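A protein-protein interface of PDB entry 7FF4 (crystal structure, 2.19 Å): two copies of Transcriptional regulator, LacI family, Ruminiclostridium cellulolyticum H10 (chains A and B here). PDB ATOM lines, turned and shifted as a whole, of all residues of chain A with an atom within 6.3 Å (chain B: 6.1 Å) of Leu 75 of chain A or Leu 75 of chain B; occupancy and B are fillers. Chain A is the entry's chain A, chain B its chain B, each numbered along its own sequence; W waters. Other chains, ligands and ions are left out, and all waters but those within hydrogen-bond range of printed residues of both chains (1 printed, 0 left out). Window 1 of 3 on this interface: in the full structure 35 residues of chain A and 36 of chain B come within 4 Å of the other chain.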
ATOM      1  N   PHE A  69       1.399   7.659 -20.924  1.00  0.00           N
ATOM      2  CA  PHE A  69       2.807   8.050 -21.128  1.00  0.00           C
ATOM      3  C   PHE A  69       2.807   9.560 -21.337  1.00  0.00           C
ATOM      4  O   PHE A  69       2.074  10.014 -22.165  1.00  0.00           O
ATOM      5  CB  PHE A  69       3.359   7.339 -22.354  1.00  0.00           C
ATOM      6  CG  PHE A  69       3.678   5.889 -22.133  1.00  0.00           C
ATOM      7  CD1 PHE A  69       4.750   5.510 -21.360  1.00  0.00           C
ATOM      8  CD2 PHE A  69       2.896   4.904 -22.688  1.00  0.00           C
ATOM      9  CE1 PHE A  69       5.038   4.176 -21.155  1.00  0.00           C
ATOM     10  CE2 PHE A  69       3.191   3.570 -22.489  1.00  0.00           C
ATOM     11  CZ  PHE A  69       4.262   3.207 -21.725  1.00  0.00           C
ATOM     12  N   ASN A  70       3.571  10.303 -20.556  1.00  0.00           N
ATOM     13  CA  ASN A  70       3.591  11.777 -20.727  1.00  0.00           C
ATOM     14  C   ASN A  70       4.972  12.315 -20.377  1.00  0.00           C
ATOM     15  O   ASN A  70       5.751  11.586 -19.805  1.00  0.00           O
ATOM     16  CB  ASN A  70       2.491  12.462 -19.931  1.00  0.00           C
ATOM     17  CG  ASN A  70       2.631  12.235 -18.448  1.00  0.00           C
ATOM     18  OD1 ASN A  70       3.710  11.955 -17.959  1.00  0.00           O
ATOM     19  ND2 ASN A  70       1.541  12.361 -17.726  1.00  0.00           N
ATOM     20  N   ALA A  71       5.235  13.563 -20.727  1.00  0.00           N
ATOM     21  CA  ALA A  71       6.556  14.165 -20.473  1.00  0.00           C
ATOM     22  C   ALA A  71       6.567  14.811 -19.095  1.00  0.00           C
ATOM     23  O   ALA A  71       6.621  16.008 -19.011  1.00  0.00           O
ATOM     24  CB  ALA A  71       6.859  15.168 -21.544  1.00  0.00           C
ATOM     25  N   SER A  72       6.458  14.013 -18.057  1.00  0.00           N
ATOM     26  CA  SER A  72       6.516  14.583 -16.697  1.00  0.00           C
ATOM     27  C   SER A  72       7.789  14.098 -16.021  1.00  0.00           C
ATOM     28  O   SER A  72       8.587  13.427 -16.654  1.00  0.00           O
ATOM     29  CB  SER A  72       5.310  14.202 -15.916  1.00  0.00           C
ATOM     30  OG  SER A  72       5.349  12.838 -15.587  1.00  0.00           O
ATOM     31  N   VAL A  73       7.930  14.415 -14.737  1.00  0.00           N
ATOM     32  CA  VAL A  73       9.108  13.993 -13.928  1.00  0.00           C
ATOM     33  C   VAL A  73       9.100  12.470 -13.828  1.00  0.00           C
ATOM     34  O   VAL A  73      10.157  11.889 -13.673  1.00  0.00           O
ATOM     35  CB  VAL A  73       9.064  14.602 -12.520  1.00  0.00           C
ATOM     36  CG1 VAL A  73       9.724  15.960 -12.463  1.00  0.00           C
ATOM     37  CG2 VAL A  73       7.647  14.670 -11.994  1.00  0.00           C
ATOM     38  N   TYR A  74       7.920  11.872 -13.956  1.00  0.00           N
ATOM     39  CA  TYR A  74       7.743  10.406 -13.849  1.00  0.00           C
ATOM     40  C   TYR A  74       8.491   9.666 -14.951  1.00  0.00           C
ATOM     41  O   TYR A  74       8.704   8.477 -14.816  1.00  0.00           O
ATOM     42  CB  TYR A  74       6.262  10.056 -13.804  1.00  0.00           C
ATOM     43  CG  TYR A  74       5.645  10.415 -12.486  1.00  0.00           C
ATOM     44  CD1 TYR A  74       5.986   9.732 -11.341  1.00  0.00           C
ATOM     45  CD2 TYR A  74       4.765  11.469 -12.372  1.00  0.00           C
ATOM     46  CE1 TYR A  74       5.444  10.066 -10.117  1.00  0.00           C
ATOM     47  CE2 TYR A  74       4.208  11.814 -11.156  1.00  0.00           C
ATOM     48  CZ  TYR A  74       4.555  11.111 -10.023  1.00  0.00           C
ATOM     49  OH  TYR A  74       4.027  11.443  -8.817  1.00  0.00           O
ATOM     50  N   LEU A  75       8.876  10.372 -16.006  1.00  0.00           N
ATOM     51  CA  LEU A  75       9.645   9.745 -17.101  1.00  0.00           C
ATOM     52  C   LEU A  75      10.976   9.272 -16.527  1.00  0.00           C
ATOM     53  O   LEU A  75      11.393   8.183 -16.840  1.00  0.00           O
ATOM     54  CB  LEU A  75       9.878  10.804 -18.173  1.00  0.00           C
ATOM     55  CG  LEU A  75       9.618  10.379 -19.607  1.00  0.00           C
ATOM     56  CD1 LEU A  75       8.421   9.462 -19.696  1.00  0.00           C
ATOM     57  CD2 LEU A  75       9.419  11.593 -20.484  1.00  0.00           C
ATOM     58  N   LYS A  76      11.606  10.093 -15.696  1.00  0.00           N
ATOM     59  CA  LYS A  76      12.916   9.715 -15.122  1.00  0.00           C
ATOM     60  C   LYS A  76      12.713   8.591 -14.113  1.00  0.00           C
ATOM     61  O   LYS A  76      13.585   7.774 -13.992  1.00  0.00           O
ATOM     62  CB  LYS A  76      13.624  10.928 -14.519  1.00  0.00           C
ATOM     63  CG  LYS A  76      14.050  11.994 -15.518  1.00  0.00           C
ATOM     64  CD  LYS A  76      15.004  11.533 -16.610  1.00  0.00           C
ATOM     65  CE  LYS A  76      14.329  10.931 -17.832  1.00  0.00           C
ATOM     66  NZ  LYS A  76      14.789  11.531 -19.108  1.00  0.00           N
ATOM     67  N   LEU A  77      11.576   8.578 -13.438  1.00  0.00           N
ATOM     68  CA  LEU A  77      11.292   7.520 -12.447  1.00  0.00           C
ATOM     69  C   LEU A  77      11.244   6.176 -13.161  1.00  0.00           C
ATOM     70  O   LEU A  77      11.826   5.261 -12.671  1.00  0.00           O
ATOM     71  CB  LEU A  77       9.946   7.820 -11.790  1.00  0.00           C
ATOM     72  CG  LEU A  77       9.792   7.354 -10.351  1.00  0.00           C
ATOM     73  CD1 LEU A  77       8.338   7.343  -9.952  1.00  0.00           C
ATOM     74  CD2 LEU A  77      10.370   5.979 -10.169  1.00  0.00           C
ATOM     75  N   ALA A  78      10.583   6.112 -14.306  1.00  0.00           N
ATOM     76  CA  ALA A  78      10.438   4.854 -15.059  1.00  0.00           C
ATOM     77  C   ALA A  78      11.799   4.255 -15.399  1.00  0.00           C
ATOM     78  O   ALA A  78      11.969   3.077 -15.195  1.00  0.00           O
ATOM     79  CB  ALA A  78       9.622   5.097 -16.287  1.00  0.00           C
ATOM     80  N   ASN A  79      12.726   5.052 -15.916  1.00  0.00           N
ATOM     81  CA  ASN A  79      14.050   4.500 -16.286  1.00  0.00           C
ATOM     82  C   ASN A  79      14.777   4.020 -15.034  1.00  0.00           C
ATOM     83  O   ASN A  79      15.435   3.005 -15.111  1.00  0.00           O
ATOM     84  CB  ASN A  79      14.883   5.484 -17.099  1.00  0.00           C
ATOM     85  CG  ASN A  79      14.263   5.802 -18.440  1.00  0.00           C
ATOM     86  OD1 ASN A  79      13.762   4.926 -19.125  1.00  0.00           O
ATOM     87  ND2 ASN A  79      14.273   7.065 -18.806  1.00  0.00           N
ATOM     88  N   TYR A  80      14.638   4.741 -13.931  1.00  0.00           N
ATOM     89  CA  TYR A  80      15.324   4.351 -12.679  1.00  0.00           C
ATOM     90  C   TYR A  80      14.720   3.063 -12.139  1.00  0.00           C
ATOM     91  O   TYR A  80      15.444   2.300 -11.550  1.00  0.00           O
ATOM     92  CB  TYR A  80      15.282   5.473 -11.650  1.00  0.00           C
ATOM     93  CG  TYR A  80      16.203   6.627 -11.923  1.00  0.00           C
ATOM     94  CD1 TYR A  80      17.551   6.443 -12.151  1.00  0.00           C
ATOM     95  CD2 TYR A  80      15.711   7.910 -11.948  1.00  0.00           C
ATOM     96  CE1 TYR A  80      18.393   7.509 -12.394  1.00  0.00           C
ATOM     97  CE2 TYR A  80      16.533   8.987 -12.192  1.00  0.00           C
ATOM     98  CZ  TYR A  80      17.875   8.786 -12.417  1.00  0.00           C
ATOM     99  OH  TYR A  80      18.654   9.865 -12.664  1.00  0.00           O
ATOM    100  N   ILE A 279      14.423  16.924 -18.310  1.00  0.00           N
ATOM    101  CA  ILE A 279      13.980  15.985 -19.371  1.00  0.00           C
ATOM    102  C   ILE A 279      14.077  16.655 -20.741  1.00  0.00           C
ATOM    103  O   ILE A 279      13.703  16.030 -21.714  1.00  0.00           O
ATOM    104  CB  ILE A 279      12.595  15.402 -19.067  1.00  0.00           C
ATOM    105  CG1 ILE A 279      11.473  16.384 -19.384  1.00  0.00           C
ATOM    106  CG2 ILE A 279      12.527  14.937 -17.631  1.00  0.00           C
ATOM    107  CD1 ILE A 279      10.118  15.737 -19.424  1.00  0.00           C
ATOM    108  N   PHE B  69      12.932   5.594 -21.753  1.00  0.00           N
ATOM    109  CA  PHE B  69      11.779   6.510 -21.710  1.00  0.00           C
ATOM    110  C   PHE B  69      12.382   7.903 -21.821  1.00  0.00           C
ATOM    111  O   PHE B  69      13.321   8.170 -21.122  1.00  0.00           O
ATOM    112  CB  PHE B  69      11.018   6.344 -20.401  1.00  0.00           C
ATOM    113  CG  PHE B  69      10.155   5.117 -20.340  1.00  0.00           C
ATOM    114  CD1 PHE B  69       9.006   5.028 -21.090  1.00  0.00           C
ATOM    115  CD2 PHE B  69      10.503   4.045 -19.548  1.00  0.00           C
ATOM    116  CE1 PHE B  69       8.218   3.894 -21.043  1.00  0.00           C
ATOM    117  CE2 PHE B  69       9.712   2.916 -19.495  1.00  0.00           C
ATOM    118  CZ  PHE B  69       8.572   2.841 -20.244  1.00  0.00           C
ATOM    119  N   ASN B  70      11.897   8.699 -22.748  1.00  0.00           N
ATOM    120  CA  ASN B  70      12.374  10.085 -22.962  1.00  0.00           C
ATOM    121  C   ASN B  70      11.229  10.892 -23.561  1.00  0.00           C
ATOM    122  O   ASN B  70      10.268  10.295 -24.023  1.00  0.00           O
ATOM    123  CB  ASN B  70      13.606  10.115 -23.855  1.00  0.00           C
ATOM    124  CG  ASN B  70      13.326   9.509 -25.206  1.00  0.00           C
ATOM    125  OD1 ASN B  70      12.212   9.577 -25.709  1.00  0.00           O
ATOM    126  ND2 ASN B  70      14.333   8.899 -25.788  1.00  0.00           N
ATOM    127  N   ALA B  71      11.353  12.211 -23.593  1.00  0.00           N
ATOM    128  CA  ALA B  71      10.247  13.054 -24.082  1.00  0.00           C
ATOM    129  C   ALA B  71      10.290  13.222 -25.599  1.00  0.00           C
ATOM    130  O   ALA B  71      10.234  14.337 -26.054  1.00  0.00           O
ATOM    131  CB  ALA B  71      10.280  14.379 -23.382  1.00  0.00           C
ATOM    132  N   SER B  72      10.370  12.141 -26.345  1.00  0.00           N
ATOM    133  CA  SER B  72      10.383  12.302 -27.813  1.00  0.00           C
ATOM    134  C   SER B  72       8.967  12.165 -28.350  1.00  0.00           C
ATOM    135  O   SER B  72       8.049  11.994 -27.578  1.00  0.00           O
ATOM    136  CB  SER B  72      11.273  11.297 -28.443  1.00  0.00           C
ATOM    137  OG  SER B  72      10.644  10.040 -28.443  1.00  0.00           O
ATOM    138  N   VAL B  73       8.838  12.196 -29.670  1.00  0.00           N
ATOM    139  CA  VAL B  73       7.521  12.054 -30.348  1.00  0.00           C
ATOM    140  C   VAL B  73       6.989  10.645 -30.105  1.00  0.00           C
ATOM    141  O   VAL B  73       5.800  10.479 -30.169  1.00  0.00           O
ATOM    142  CB  VAL B  73       7.625  12.327 -31.856  1.00  0.00           C
ATOM    143  CG1 VAL B  73       7.626  13.804 -32.166  1.00  0.00           C
ATOM    144  CG2 VAL B  73       8.832  11.650 -32.472  1.00  0.00           C
ATOM    145  N   TYR B  74       7.865   9.696 -29.779  1.00  0.00           N
ATOM    146  CA  TYR B  74       7.463   8.282 -29.565  1.00  0.00           C
ATOM    147  C   TYR B  74       6.570   8.138 -28.341  1.00  0.00           C
ATOM    148  O   TYR B  74       5.893   7.136 -28.232  1.00  0.00           O
ATOM    149  CB  TYR B  74       8.673   7.358 -29.509  1.00  0.00           C
ATOM    150  CG  TYR B  74       9.345   7.186 -30.841  1.00  0.00           C
ATOM    151  CD1 TYR B  74       8.687   6.595 -31.893  1.00  0.00           C
ATOM    152  CD2 TYR B  74      10.619   7.656 -31.061  1.00  0.00           C
ATOM    153  CE1 TYR B  74       9.284   6.450 -33.128  1.00  0.00           C
ATOM    154  CE2 TYR B  74      11.232   7.524 -32.293  1.00  0.00           C
ATOM    155  CZ  TYR B  74      10.563   6.915 -33.331  1.00  0.00           C
ATOM    156  OH  TYR B  74      11.162   6.781 -34.545  1.00  0.00           O
ATOM    157  N   LEU B  75       6.577   9.129 -27.457  1.00  0.00           N
ATOM    158  CA  LEU B  75       5.699   9.104 -26.268  1.00  0.00           C
ATOM    159  C   LEU B  75       4.259   9.114 -26.763  1.00  0.00           C
ATOM    160  O   LEU B  75       3.462   8.391 -26.225  1.00  0.00           O
ATOM    161  CB  LEU B  75       5.976  10.355 -25.442  1.00  0.00           C
ATOM    162  CG  LEU B  75       6.269  10.135 -23.965  1.00  0.00           C
ATOM    163  CD1 LEU B  75       7.179   8.942 -23.759  1.00  0.00           C
ATOM    164  CD2 LEU B  75       6.890  11.383 -23.383  1.00  0.00           C
ATOM    165  N   LYS B  76       3.962   9.937 -27.760  1.00  0.00           N
ATOM    166  CA  LYS B  76       2.589   9.972 -28.316  1.00  0.00           C
ATOM    167  C   LYS B  76       2.314   8.642 -29.016  1.00  0.00           C
ATOM    168  O   LYS B  76       1.220   8.131 -28.896  1.00  0.00           O
ATOM    169  CB  LYS B  76       2.432  11.131 -29.300  1.00  0.00           C
ATOM    170  CG  LYS B  76       1.256  12.053 -29.020  1.00  0.00           C
ATOM    171  CD  LYS B  76       0.631  12.616 -30.267  1.00  0.00           C
ATOM    172  CE  LYS B  76      -0.332  13.749 -29.999  1.00  0.00           C
ATOM    173  NZ  LYS B  76      -0.935  14.270 -31.247  1.00  0.00           N
ATOM    174  N   LEU B  77       3.312   8.115 -29.711  1.00  0.00           N
ATOM    175  CA  LEU B  77       3.150   6.832 -30.427  1.00  0.00           C
ATOM    176  C   LEU B  77       2.774   5.742 -29.424  1.00  0.00           C
ATOM    177  O   LEU B  77       1.875   4.985 -29.712  1.00  0.00           O
ATOM    178  CB  LEU B  77       4.458   6.499 -31.138  1.00  0.00           C
ATOM    179  CG  LEU B  77       4.408   5.274 -32.039  1.00  0.00           C
ATOM    180  CD1 LEU B  77       3.315   5.420 -33.069  1.00  0.00           C
ATOM    181  CD2 LEU B  77       5.736   5.049 -32.718  1.00  0.00           C
ATOM    182  N   ALA B  78       3.443   5.709 -28.278  1.00  0.00           N
ATOM    183  CA  ALA B  78       3.176   4.691 -27.243  1.00  0.00           C
ATOM    184  C   ALA B  78       1.710   4.732 -26.815  1.00  0.00           C
ATOM    185  O   ALA B  78       1.098   3.692 -26.813  1.00  0.00           O
ATOM    186  CB  ALA B  78       4.100   4.875 -26.080  1.00  0.00           C
ATOM    187  N   ASN B  79       1.164   5.899 -26.500  1.00  0.00           N
ATOM    188  CA  ASN B  79      -0.248   5.945 -26.060  1.00  0.00           C
ATOM    189  C   ASN B  79      -1.168   5.477 -27.181  1.00  0.00           C
ATOM    190  O   ASN B  79      -2.152   4.829 -26.898  1.00  0.00           O
ATOM    191  CB  ASN B  79      -0.642   7.336 -25.594  1.00  0.00           C
ATOM    192  CG  ASN B  79       0.028   7.692 -24.293  1.00  0.00           C
ATOM    193  OD1 ASN B  79       0.117   6.876 -23.390  1.00  0.00           O
ATOM    194  ND2 ASN B  79       0.521   8.907 -24.206  1.00  0.00           N
ATOM    195  N   TYR B  80      -0.841   5.829 -28.412  1.00  0.00           N
ATOM    196  CA  TYR B  80      -1.701   5.467 -29.560  1.00  0.00           C
ATOM    197  C   TYR B  80      -1.668   3.958 -29.796  1.00  0.00           C
ATOM    198  O   TYR B  80      -2.665   3.419 -30.222  1.00  0.00           O
ATOM    199  CB  TYR B  80      -1.321   6.311 -30.771  1.00  0.00           C
ATOM    200  CG  TYR B  80      -1.910   7.694 -30.784  1.00  0.00           C
ATOM    201  CD1 TYR B  80      -3.241   7.911 -30.499  1.00  0.00           C
ATOM    202  CD2 TYR B  80      -1.141   8.785 -31.115  1.00  0.00           C
ATOM    203  CE1 TYR B  80      -3.789   9.177 -30.527  1.00  0.00           C
ATOM    204  CE2 TYR B  80      -1.669  10.059 -31.151  1.00  0.00           C
ATOM    205  CZ  TYR B  80      -3.000  10.256 -30.856  1.00  0.00           C
ATOM    206  OH  TYR B  80      -3.519  11.511 -30.891  1.00  0.00           O
ATOM    207  N   ILE B 279       4.135  17.421 -27.155  1.00  0.00           N
ATOM    208  CA  ILE B 279       4.567  16.423 -26.143  1.00  0.00           C
ATOM    209  C   ILE B 279       4.576  17.065 -24.756  1.00  0.00           C
ATOM    210  O   ILE B 279       4.050  16.473 -23.840  1.00  0.00           O
ATOM    211  CB  ILE B 279       5.956  15.893 -26.511  1.00  0.00           C
ATOM    212  CG1 ILE B 279       5.951  15.224 -27.880  1.00  0.00           C
ATOM    213  CG2 ILE B 279       6.484  14.964 -25.447  1.00  0.00           C
ATOM    214  CD1 ILE B 279       7.269  15.338 -28.586  1.00  0.00           C
HETATM  215  O   HOH W   1      13.859  13.234 -22.187  1.00  0.00           O
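The backbone carbonyl oxygen (O) of Phe 69 of chain A lies within hydrogen-bond range of the side-chain amide nitrogen (ND2) of Asn 79 of chain B (2.8 Å).
The backbone carbonyl oxygen (O) of Phe 69 of chain B is in hydrogen-bond range of the side-chain amide nitrogen (ND2) of Asn 79 of chain A (2.7 Å).
The side-chain amide oxygen of Asn 70 of chain A lies within hydrogen-bond range of the side-chain hydroxyl of Ser 72 of chain A.
The side-chain amide oxygen (OD1) of Asn 70 of chain B lies within hydrogen-bond range of the side-chain hydroxyl (OG) of Ser 72 of chain B (3.2 Å).
CE1 of Phe 69 of chain A touches CE1 of Phe 69 of chain B, 3.2 Å away.
Ala 78 of chain B touches Phe 69 of chain A (CB to CD2, 3.6 Å).
Asn 70 of chain A touches Leu 75 of chain B.
Ala 71 of chain A touches Ala 71 of chain B.
Leu 75 of chain B touches Ala 71 of chain A (CD2 to N, 3.8 Å).
Ala 71 of chain A touches Ile 279 of chain B.
C of Asn 70 of chain B touches CD2 of Leu 75 of chain A (3.6 Å).
Ala 71 of chain B touches Leu 75 of chain A (N to CD2, 3.7 Å).
Leu 75 of chain A touches Leu 75 of chain B.
CB of Ala 78 of chain A touches CD2 of Phe 69 of chain B, at 3.5 Å.
Printed residues of chain B within 4 Å of Phe 69 of chain A: Phe 69 (3.2 Å), Ala 78 (3.6 Å) and Asn 79 (2.8 Å).
Tyr 80 of chain A touches none of the printed residues of chain B.
Of the printed residues of chain A, Phe 69 of chain B touches Phe 69 (3.2 Å), Ala 78 (3.5 Å) and Asn 79 (2.7 Å).
Printed residues of chain A within 4 Å of Leu 75 of chain B: Asn 70 (3.7 Å), Ala 71 (3.8 Å) and Leu 75 (3.9 Å).
Of the printed residues of chain A, Ala 78 of chain B touches Phe 69 (3.6 Å).
Tyr 80 of chain B touches none of the printed residues of chain A.
The nearest residue of chain B that does not touch Leu 75 of chain A is Phe 69 of chain B (4.03 Å).
The nearest printed residue of chain A that does not touch Leu 75 of chain B is Phe 69 of chain A (4.01 Å).
Of the 13 printed residues of chain B, 7 touch a printed residue of chain A.
Of the 13 printed residues of chain A, 6 touch a printed residue of chain B.
Among the printed residues, 12 pairs touch across the chains.
Among the printed residues, no Asp or Glu carboxylate lies within 4 Å of a Lys or Arg side-chain nitrogen of the other chain.
Phe 69 of chain A touches Ala 78 of chain B, and with the chains exchanged Ala 78 of chain A touches Phe 69 of chain B.
Ala 71 of chain A touches its own counterpart, Ala 71 of chain B.
Ala 71 of chain A touches Ile 279 of chain B, but with the chains exchanged Ile 279 of chain A does not touch Ala 71 of chain B (4.2 Å).
Leu 75 of chain B touches its own counterpart, Leu 75 of chain A.
Of the 12 pairs that touch across the chains among the printed residues, 11 have their exchanged pair printed and touching as well.
Water W1 lies within hydrogen-bond range of the backbone carbonyl oxygen of Ile 279 of chain A and the backbone NH of Ala 71 of chain B.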
